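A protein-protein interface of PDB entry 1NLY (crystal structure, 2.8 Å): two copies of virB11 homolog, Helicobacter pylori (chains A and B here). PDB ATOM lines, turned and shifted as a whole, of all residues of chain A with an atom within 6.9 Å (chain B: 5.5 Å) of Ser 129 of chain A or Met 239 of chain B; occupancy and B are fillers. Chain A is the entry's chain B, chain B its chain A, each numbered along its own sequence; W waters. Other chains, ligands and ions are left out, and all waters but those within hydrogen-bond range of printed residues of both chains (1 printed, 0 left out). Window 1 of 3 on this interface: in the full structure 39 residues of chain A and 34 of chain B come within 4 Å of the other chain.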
ATOM      1  N   GLU A  47      11.839 -40.362  23.272  1.00  0.00           N
ATOM      2  CA  GLU A  47      12.189 -39.191  24.071  1.00  0.00           C
ATOM      3  C   GLU A  47      11.546 -39.285  25.443  1.00  0.00           C
ATOM      4  O   GLU A  47      10.497 -39.908  25.605  1.00  0.00           O
ATOM      5  CB  GLU A  47      11.686 -37.927  23.377  1.00  0.00           C
ATOM      6  CG  GLU A  47      12.164 -36.608  23.949  1.00  0.00           C
ATOM      7  CD  GLU A  47      13.486 -36.146  23.368  1.00  0.00           C
ATOM      8  OE1 GLU A  47      13.863 -36.548  22.245  1.00  0.00           O
ATOM      9  OE2 GLU A  47      14.149 -35.342  24.038  1.00  0.00           O
ATOM     10  N   CYS A  49      10.596 -36.543  28.349  1.00  0.00           N
ATOM     11  CA  CYS A  49      10.633 -35.149  28.761  1.00  0.00           C
ATOM     12  C   CYS A  49      10.062 -34.920  30.163  1.00  0.00           C
ATOM     13  O   CYS A  49       9.250 -35.708  30.652  1.00  0.00           O
ATOM     14  CB  CYS A  49       9.866 -34.302  27.758  1.00  0.00           C
ATOM     15  SG  CYS A  49      10.621 -34.293  26.128  1.00  0.00           S
ATOM     16  N   TYR A  50      10.515 -33.851  30.814  1.00  0.00           N
ATOM     17  CA  TYR A  50      10.012 -33.481  32.130  1.00  0.00           C
ATOM     18  C   TYR A  50       9.814 -31.979  32.102  1.00  0.00           C
ATOM     19  O   TYR A  50      10.746 -31.221  31.810  1.00  0.00           O
ATOM     20  CB  TYR A  50      10.967 -33.862  33.240  1.00  0.00           C
ATOM     21  CG  TYR A  50      10.356 -33.601  34.605  1.00  0.00           C
ATOM     22  CD1 TYR A  50       9.180 -34.244  35.008  1.00  0.00           C
ATOM     23  CD2 TYR A  50      10.926 -32.667  35.479  1.00  0.00           C
ATOM     24  CE1 TYR A  50       8.575 -33.952  36.268  1.00  0.00           C
ATOM     25  CE2 TYR A  50      10.339 -32.359  36.730  1.00  0.00           C
ATOM     26  CZ  TYR A  50       9.167 -33.000  37.120  1.00  0.00           C
ATOM     27  OH  TYR A  50       8.593 -32.660  38.327  1.00  0.00           O
ATOM     28  N   ASN A  51       8.599 -31.554  32.417  1.00  0.00           N
ATOM     29  CA  ASN A  51       8.267 -30.148  32.337  1.00  0.00           C
ATOM     30  C   ASN A  51       8.118 -29.523  33.722  1.00  0.00           C
ATOM     31  O   ASN A  51       7.327 -28.587  33.936  1.00  0.00           O
ATOM     32  CB  ASN A  51       6.984 -30.001  31.507  1.00  0.00           C
ATOM     33  CG  ASN A  51       6.993 -30.860  30.234  1.00  0.00           C
ATOM     34  OD1 ASN A  51       5.947 -31.124  29.667  1.00  0.00           O
ATOM     35  ND2 ASN A  51       8.166 -31.283  29.791  1.00  0.00           N
ATOM     36  N   GLY A  52       8.921 -30.045  34.646  1.00  0.00           N
ATOM     37  CA  GLY A  52       8.953 -29.566  36.024  1.00  0.00           C
ATOM     38  C   GLY A  52       7.590 -29.298  36.611  1.00  0.00           C
ATOM     39  O   GLY A  52       7.392 -28.332  37.354  1.00  0.00           O
ATOM     40  N   TRP A  65       2.335 -39.561  22.711  1.00  0.00           N
ATOM     41  CA  TRP A  65       2.891 -39.012  23.941  1.00  0.00           C
ATOM     42  C   TRP A  65       2.146 -39.636  25.081  1.00  0.00           C
ATOM     43  O   TRP A  65       0.909 -39.623  25.093  1.00  0.00           O
ATOM     44  CB  TRP A  65       2.688 -37.504  24.034  1.00  0.00           C
ATOM     45  CG  TRP A  65       3.674 -36.693  23.281  1.00  0.00           C
ATOM     46  CD1 TRP A  65       3.479 -36.008  22.136  1.00  0.00           C
ATOM     47  CD2 TRP A  65       5.067 -36.491  23.632  1.00  0.00           C
ATOM     48  NE1 TRP A  65       4.661 -35.386  21.738  1.00  0.00           N
ATOM     49  CE2 TRP A  65       5.667 -35.672  22.654  1.00  0.00           C
ATOM     50  CE3 TRP A  65       5.877 -36.936  24.697  1.00  0.00           C
ATOM     51  CZ2 TRP A  65       7.002 -35.280  22.682  1.00  0.00           C
ATOM     52  CZ3 TRP A  65       7.254 -36.550  24.746  1.00  0.00           C
ATOM     53  CH2 TRP A  65       7.773 -35.720  23.716  1.00  0.00           C
ATOM     54  N   GLN A 115      18.870 -32.391  27.543  1.00  0.00           N
ATOM     55  CA  GLN A 115      18.640 -30.956  27.465  1.00  0.00           C
ATOM     56  C   GLN A 115      17.986 -30.518  28.761  1.00  0.00           C
ATOM     57  O   GLN A 115      16.822 -30.864  29.015  1.00  0.00           O
ATOM     58  CB  GLN A 115      17.681 -30.641  26.327  1.00  0.00           C
ATOM     59  CG  GLN A 115      17.685 -29.195  25.874  1.00  0.00           C
ATOM     60  CD  GLN A 115      19.050 -28.739  25.413  1.00  0.00           C
ATOM     61  OE1 GLN A 115      19.939 -29.549  25.147  1.00  0.00           O
ATOM     62  NE2 GLN A 115      19.220 -27.433  25.301  1.00  0.00           N
ATOM     63  N   ILE A 116      18.715 -29.744  29.561  1.00  0.00           N
ATOM     64  CA  ILE A 116      18.208 -29.247  30.842  1.00  0.00           C
ATOM     65  C   ILE A 116      18.056 -27.737  30.867  1.00  0.00           C
ATOM     66  O   ILE A 116      18.970 -27.009  30.496  1.00  0.00           O
ATOM     67  CB  ILE A 116      19.147 -29.642  32.009  1.00  0.00           C
ATOM     68  CG1 ILE A 116      19.205 -31.163  32.140  1.00  0.00           C
ATOM     69  CG2 ILE A 116      18.692 -28.963  33.310  1.00  0.00           C
ATOM     70  CD1 ILE A 116      20.204 -31.651  33.148  1.00  0.00           C
ATOM     71  N   VAL A 117      16.898 -27.274  31.323  1.00  0.00           N
ATOM     72  CA  VAL A 117      16.631 -25.841  31.411  1.00  0.00           C
ATOM     73  C   VAL A 117      16.155 -25.400  32.814  1.00  0.00           C
ATOM     74  O   VAL A 117      15.306 -26.045  33.432  1.00  0.00           O
ATOM     75  CB  VAL A 117      15.615 -25.432  30.321  1.00  0.00           C
ATOM     76  CG1 VAL A 117      15.458 -23.934  30.285  1.00  0.00           C
ATOM     77  CG2 VAL A 117      16.090 -25.929  28.975  1.00  0.00           C
ATOM     78  N   LEU A 118      16.705 -24.299  33.319  1.00  0.00           N
ATOM     79  CA  LEU A 118      16.336 -23.852  34.654  1.00  0.00           C
ATOM     80  C   LEU A 118      15.869 -22.424  34.642  1.00  0.00           C
ATOM     81  O   LEU A 118      15.944 -21.760  33.611  1.00  0.00           O
ATOM     82  CB  LEU A 118      17.532 -23.952  35.580  1.00  0.00           C
ATOM     83  CG  LEU A 118      18.207 -25.305  35.685  1.00  0.00           C
ATOM     84  CD1 LEU A 118      19.430 -25.177  36.553  1.00  0.00           C
ATOM     85  CD2 LEU A 118      17.239 -26.295  36.276  1.00  0.00           C
ATOM     86  N   THR A 122      13.067 -21.041  32.500  1.00  0.00           N
ATOM     87  CA  THR A 122      11.819 -21.778  32.609  1.00  0.00           C
ATOM     88  C   THR A 122      10.850 -20.773  33.238  1.00  0.00           C
ATOM     89  O   THR A 122      11.283 -19.791  33.836  1.00  0.00           O
ATOM     90  CB  THR A 122      11.956 -23.029  33.541  1.00  0.00           C
ATOM     91  OG1 THR A 122      12.281 -22.623  34.877  1.00  0.00           O
ATOM     92  CG2 THR A 122      13.047 -23.953  33.054  1.00  0.00           C
ATOM     93  N   THR A 127      10.258 -24.925  38.182  1.00  0.00           N
ATOM     94  CA  THR A 127      10.201 -25.649  36.936  1.00  0.00           C
ATOM     95  C   THR A 127      11.592 -25.970  36.429  1.00  0.00           C
ATOM     96  O   THR A 127      12.403 -25.083  36.163  1.00  0.00           O
ATOM     97  CB  THR A 127       9.472 -24.846  35.891  1.00  0.00           C
ATOM     98  OG1 THR A 127       8.117 -24.675  36.320  1.00  0.00           O
ATOM     99  CG2 THR A 127       9.508 -25.550  34.542  1.00  0.00           C
ATOM    100  N   ILE A 128      11.859 -27.264  36.321  1.00  0.00           N
ATOM    101  CA  ILE A 128      13.121 -27.770  35.823  1.00  0.00           C
ATOM    102  C   ILE A 128      12.806 -28.670  34.636  1.00  0.00           C
ATOM    103  O   ILE A 128      12.324 -29.783  34.784  1.00  0.00           O
ATOM    104  CB  ILE A 128      13.883 -28.517  36.930  1.00  0.00           C
ATOM    105  CG1 ILE A 128      14.446 -27.499  37.925  1.00  0.00           C
ATOM    106  CG2 ILE A 128      15.011 -29.310  36.341  1.00  0.00           C
ATOM    107  CD1 ILE A 128      15.178 -28.113  39.075  1.00  0.00           C
ATOM    108  N   SER A 129      13.069 -28.153  33.446  1.00  0.00           N
ATOM    109  CA  SER A 129      12.799 -28.866  32.213  1.00  0.00           C
ATOM    110  C   SER A 129      13.935 -29.753  31.730  1.00  0.00           C
ATOM    111  O   SER A 129      15.038 -29.272  31.470  1.00  0.00           O
ATOM    112  CB  SER A 129      12.480 -27.868  31.123  1.00  0.00           C
ATOM    113  OG  SER A 129      12.436 -28.544  29.887  1.00  0.00           O
ATOM    114  N   ILE A 130      13.649 -31.045  31.598  1.00  0.00           N
ATOM    115  CA  ILE A 130      14.627 -32.029  31.145  1.00  0.00           C
ATOM    116  C   ILE A 130      14.051 -32.691  29.913  1.00  0.00           C
ATOM    117  O   ILE A 130      12.852 -32.967  29.858  1.00  0.00           O
ATOM    118  CB  ILE A 130      14.886 -33.129  32.197  1.00  0.00           C
ATOM    119  CG1 ILE A 130      15.456 -32.507  33.478  1.00  0.00           C
ATOM    120  CG2 ILE A 130      15.817 -34.180  31.605  1.00  0.00           C
ATOM    121  CD1 ILE A 130      15.647 -33.489  34.670  1.00  0.00           C
ATOM    122  N   SER A 131      14.907 -32.942  28.933  1.00  0.00           N
ATOM    123  CA  SER A 131      14.495 -33.562  27.691  1.00  0.00           C
ATOM    124  C   SER A 131      15.522 -34.599  27.274  1.00  0.00           C
ATOM    125  O   SER A 131      16.597 -34.259  26.775  1.00  0.00           O
ATOM    126  CB  SER A 131      14.377 -32.503  26.595  1.00  0.00           C
ATOM    127  OG  SER A 131      13.206 -31.712  26.719  1.00  0.00           O
ATOM    128  N   ARG B 200       3.200 -31.594  21.748  1.00  0.00           N
ATOM    129  CA  ARG B 200       4.077 -31.034  22.768  1.00  0.00           C
ATOM    130  C   ARG B 200       4.429 -29.686  22.179  1.00  0.00           C
ATOM    131  O   ARG B 200       4.935 -29.613  21.058  1.00  0.00           O
ATOM    132  CB  ARG B 200       5.348 -31.863  22.916  1.00  0.00           C
ATOM    133  CG  ARG B 200       6.381 -31.249  23.839  1.00  0.00           C
ATOM    134  CD  ARG B 200       7.552 -32.188  24.034  1.00  0.00           C
ATOM    135  NE  ARG B 200       8.708 -31.568  24.683  1.00  0.00           N
ATOM    136  CZ  ARG B 200       8.718 -31.113  25.937  1.00  0.00           C
ATOM    137  NH1 ARG B 200       7.630 -31.193  26.714  1.00  0.00           N
ATOM    138  NH2 ARG B 200       9.826 -30.576  26.428  1.00  0.00           N
ATOM    139  N   ILE B 202       6.337 -25.832  22.618  1.00  0.00           N
ATOM    140  CA  ILE B 202       7.364 -25.064  23.299  1.00  0.00           C
ATOM    141  C   ILE B 202       7.233 -23.632  22.803  1.00  0.00           C
ATOM    142  O   ILE B 202       7.120 -23.373  21.595  1.00  0.00           O
ATOM    143  CB  ILE B 202       8.774 -25.629  23.031  1.00  0.00           C
ATOM    144  CG1 ILE B 202       8.878 -27.015  23.664  1.00  0.00           C
ATOM    145  CG2 ILE B 202       9.840 -24.711  23.612  1.00  0.00           C
ATOM    146  CD1 ILE B 202      10.208 -27.647  23.505  1.00  0.00           C
ATOM    147  N   THR B 219       6.046 -26.578  27.381  1.00  0.00           N
ATOM    148  CA  THR B 219       7.121 -25.952  28.148  1.00  0.00           C
ATOM    149  C   THR B 219       7.393 -24.539  27.658  1.00  0.00           C
ATOM    150  O   THR B 219       7.506 -24.295  26.453  1.00  0.00           O
ATOM    151  CB  THR B 219       8.420 -26.752  28.045  1.00  0.00           C
ATOM    152  OG1 THR B 219       8.288 -27.981  28.765  1.00  0.00           O
ATOM    153  CG2 THR B 219       9.563 -25.960  28.616  1.00  0.00           C
ATOM    154  N   LEU B 221       9.694 -20.998  27.447  1.00  0.00           N
ATOM    155  CA  LEU B 221      11.063 -20.536  27.492  1.00  0.00           C
ATOM    156  C   LEU B 221      11.059 -19.018  27.471  1.00  0.00           C
ATOM    157  O   LEU B 221      10.267 -18.412  26.748  1.00  0.00           O
ATOM    158  CB  LEU B 221      11.824 -21.070  26.276  1.00  0.00           C
ATOM    159  CG  LEU B 221      12.089 -22.575  26.181  1.00  0.00           C
ATOM    160  CD1 LEU B 221      12.755 -22.934  24.864  1.00  0.00           C
ATOM    161  CD2 LEU B 221      12.964 -22.973  27.339  1.00  0.00           C
ATOM    162  N   SER B 235      17.692 -24.064  22.119  1.00  0.00           N
ATOM    163  CA  SER B 235      17.446 -25.065  23.137  1.00  0.00           C
ATOM    164  C   SER B 235      16.154 -25.741  22.761  1.00  0.00           C
ATOM    165  O   SER B 235      16.012 -26.953  22.897  1.00  0.00           O
ATOM    166  CB  SER B 235      17.306 -24.411  24.520  1.00  0.00           C
ATOM    167  OG  SER B 235      17.484 -25.349  25.571  1.00  0.00           O
ATOM    168  N   CYS B 236      15.219 -24.943  22.268  1.00  0.00           N
ATOM    169  CA  CYS B 236      13.919 -25.437  21.886  1.00  0.00           C
ATOM    170  C   CYS B 236      14.074 -26.617  20.954  1.00  0.00           C
ATOM    171  O   CYS B 236      13.523 -27.691  21.217  1.00  0.00           O
ATOM    172  CB  CYS B 236      13.137 -24.338  21.197  1.00  0.00           C
ATOM    173  SG  CYS B 236      11.599 -24.884  20.496  1.00  0.00           S
ATOM    174  N   LEU B 237      14.850 -26.434  19.891  1.00  0.00           N
ATOM    175  CA  LEU B 237      15.043 -27.496  18.924  1.00  0.00           C
ATOM    176  C   LEU B 237      15.723 -28.730  19.501  1.00  0.00           C
ATOM    177  O   LEU B 237      15.981 -29.697  18.787  1.00  0.00           O
ATOM    178  CB  LEU B 237      15.831 -26.966  17.741  1.00  0.00           C
ATOM    179  CG  LEU B 237      15.139 -25.914  16.888  1.00  0.00           C
ATOM    180  CD1 LEU B 237      16.101 -25.436  15.828  1.00  0.00           C
ATOM    181  CD2 LEU B 237      13.893 -26.502  16.271  1.00  0.00           C
ATOM    182  N   ARG B 238      16.002 -28.707  20.799  1.00  0.00           N
ATOM    183  CA  ARG B 238      16.646 -29.841  21.457  1.00  0.00           C
ATOM    184  C   ARG B 238      15.707 -30.432  22.507  1.00  0.00           C
ATOM    185  O   ARG B 238      16.058 -31.354  23.254  1.00  0.00           O
ATOM    186  CB  ARG B 238      17.934 -29.388  22.130  1.00  0.00           C
ATOM    187  CG  ARG B 238      18.829 -28.555  21.248  1.00  0.00           C
ATOM    188  CD  ARG B 238      20.192 -29.197  21.128  1.00  0.00           C
ATOM    189  NE  ARG B 238      21.182 -28.183  20.794  1.00  0.00           N
ATOM    190  CZ  ARG B 238      22.492 -28.404  20.771  1.00  0.00           C
ATOM    191  NH1 ARG B 238      22.977 -29.612  21.060  1.00  0.00           N
ATOM    192  NH2 ARG B 238      23.318 -27.416  20.460  1.00  0.00           N
ATOM    193  N   MET B 239      14.491 -29.908  22.540  1.00  0.00           N
ATOM    194  CA  MET B 239      13.514 -30.357  23.505  1.00  0.00           C
ATOM    195  C   MET B 239      12.341 -31.074  22.880  1.00  0.00           C
ATOM    196  O   MET B 239      11.282 -31.128  23.479  1.00  0.00           O
ATOM    197  CB  MET B 239      13.032 -29.162  24.304  1.00  0.00           C
ATOM    198  CG  MET B 239      14.131 -28.608  25.162  1.00  0.00           C
ATOM    199  SD  MET B 239      13.854 -26.806  25.584  1.00  0.00           S
ATOM    200  CE  MET B 239      12.765 -26.962  27.166  1.00  0.00           C
ATOM    201  N   ARG B 240      12.540 -31.597  21.670  1.00  0.00           N
ATOM    202  CA  ARG B 240      11.532 -32.364  20.921  1.00  0.00           C
ATOM    203  C   ARG B 240      10.126 -31.757  20.834  1.00  0.00           C
ATOM    204  O   ARG B 240       9.146 -32.374  21.245  1.00  0.00           O
ATOM    205  CB  ARG B 240      11.423 -33.779  21.517  1.00  0.00           C
ATOM    206  CG  ARG B 240      10.482 -34.723  20.784  1.00  0.00           C
ATOM    207  CD  ARG B 240      11.069 -35.206  19.461  1.00  0.00           C
ATOM    208  NE  ARG B 240      12.096 -36.238  19.635  1.00  0.00           N
ATOM    209  CZ  ARG B 240      12.030 -37.450  19.081  1.00  0.00           C
ATOM    210  NH1 ARG B 240      10.989 -37.779  18.318  1.00  0.00           N
ATOM    211  NH2 ARG B 240      12.990 -38.348  19.293  1.00  0.00           N
ATOM    212  N   PRO B 241      10.000 -30.563  20.253  1.00  0.00           N
ATOM    213  CA  PRO B 241       8.706 -29.893  20.124  1.00  0.00           C
ATOM    214  C   PRO B 241       7.879 -30.358  18.944  1.00  0.00           C
ATOM    215  O   PRO B 241       8.432 -30.743  17.922  1.00  0.00           O
ATOM    216  CB  PRO B 241       9.109 -28.445  19.965  1.00  0.00           C
ATOM    217  CG  PRO B 241      10.320 -28.566  19.138  1.00  0.00           C
ATOM    218  CD  PRO B 241      11.082 -29.705  19.751  1.00  0.00           C
HETATM  219  O   HOH W   1      10.412 -29.931  28.713  1.00  0.00           O
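OG of Ser 235 of chain B is in hydrogen-bond range of NE2 of Gln 115 of chain A.
NE of Arg 240 of chain B is in salt-bridge range of OE1 of Glu 47 of chain A.
ND2 of Asn 51 of chain A lies within hydrogen-bond range of OG1 of Thr 219 of chain B (3.5 Å).
ND2 of Asn 51 of chain A lies close to NH1 of Arg 200 of chain B (3.1 Å).
The guanidinium group of Arg 200 of chain B is in hydrogen-bond range of the side-chain sulfur of Cys 49 of chain A, at 3.6 Å.
CZ2 of Trp 65 of chain A touches CD of Arg 200 of chain B, 3.4 Å away.
Trp 65 of chain A touches Arg 240 of chain B (CZ2 to O, 3.9 Å).
Gln 115 of chain A touches Arg 238 of chain B.
Gln 115 of chain A touches Met 239 of chain B (CG to CG, 3.7 Å).
Leu 221 of chain B touches Val 117 of chain A.
Val 117 of chain A touches Ser 235 of chain B.
Met 239 of chain B touches Val 117 of chain A.
Ser 129 of chain A touches Met 239 of chain B (OG to CE, 3.2 Å).
NH2 of Arg 200 of chain B touches OG of Ser 131 of chain A (3.6 Å).
CA of Met 239 of chain B touches OG of Ser 131 of chain A, 3.5 Å away.
No position is printed for both chains.
Hydrophobic or aromatic side chains of chain A that line the printed part of chain B: Trp 65 and Val 117.
Of the 11 printed residues of chain B, 7 touch a printed residue of chain A.
Hydrophobic or aromatic side chains of chain B that line the printed part of chain A: Leu 221 and Met 239.
Along chain B the printed residues that touch a printed residue of chain A span positions 200 to 240.
Water W1 lies within hydrogen-bond range of the guanidinium group (NH2) of Arg 200 of chain B (2.4 Å), the side-chain hydroxyl (OG) of Ser 129 of chain A (2.7 Å), the side-chain amide nitrogen (ND2) of Asn 51 of chain A (2.8 Å), the side-chain hydroxyl (OG1) of Thr 219 of chain B (2.9 Å) and the backbone carbonyl oxygen (O) of Tyr 50 of chain A (3.4 Å).
Of the printed residues of chain B, Glu 47 of chain A touches Arg 240 (3.2 Å).
Of the printed residues of chain B, Cys 49 of chain A touches Arg 200 (3.6 Å).
Ser 129 of chain A touches just one residue of chain B: Met 239.
Of the printed residues of chain A, Arg 200 of chain B touches Cys 49, Asn 51, Trp 65 and Ser 131.
Of the printed residues of chain A, Thr 219 of chain B touches Asn 51.
Of the printed residues of chain A, Leu 221 of chain B touches Val 117 (3.98 Å).
The nearest residue of chain B that does not touch Ser 129 of chain A is Thr 219 of chain B (4.1 Å).
The nearest residue of chain A that does not touch Met 239 of chain B is Cys 49 of chain A (4.2 Å).
The backbone carbonyl oxygen of Ser 129 of chain A is in hydrogen-bond range of the backbone NH of Val 117 of chain A (2.7 Å).
The guanidinium group (NE) of Arg 200 of chain B lies within hydrogen-bond range of the backbone carbonyl oxygen (O) of Met 239 of chain B (2.9 Å).
The backbone carbonyl oxygen (O) of Gln 115 of chain A is in hydrogen-bond range of the backbone NH (N) of Ser 131 of chain A (2.8 Å).
SG of Cys 49 of chain A lies within hydrogen-bond range of OG of Ser 131 of chain A (3.7 Å).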
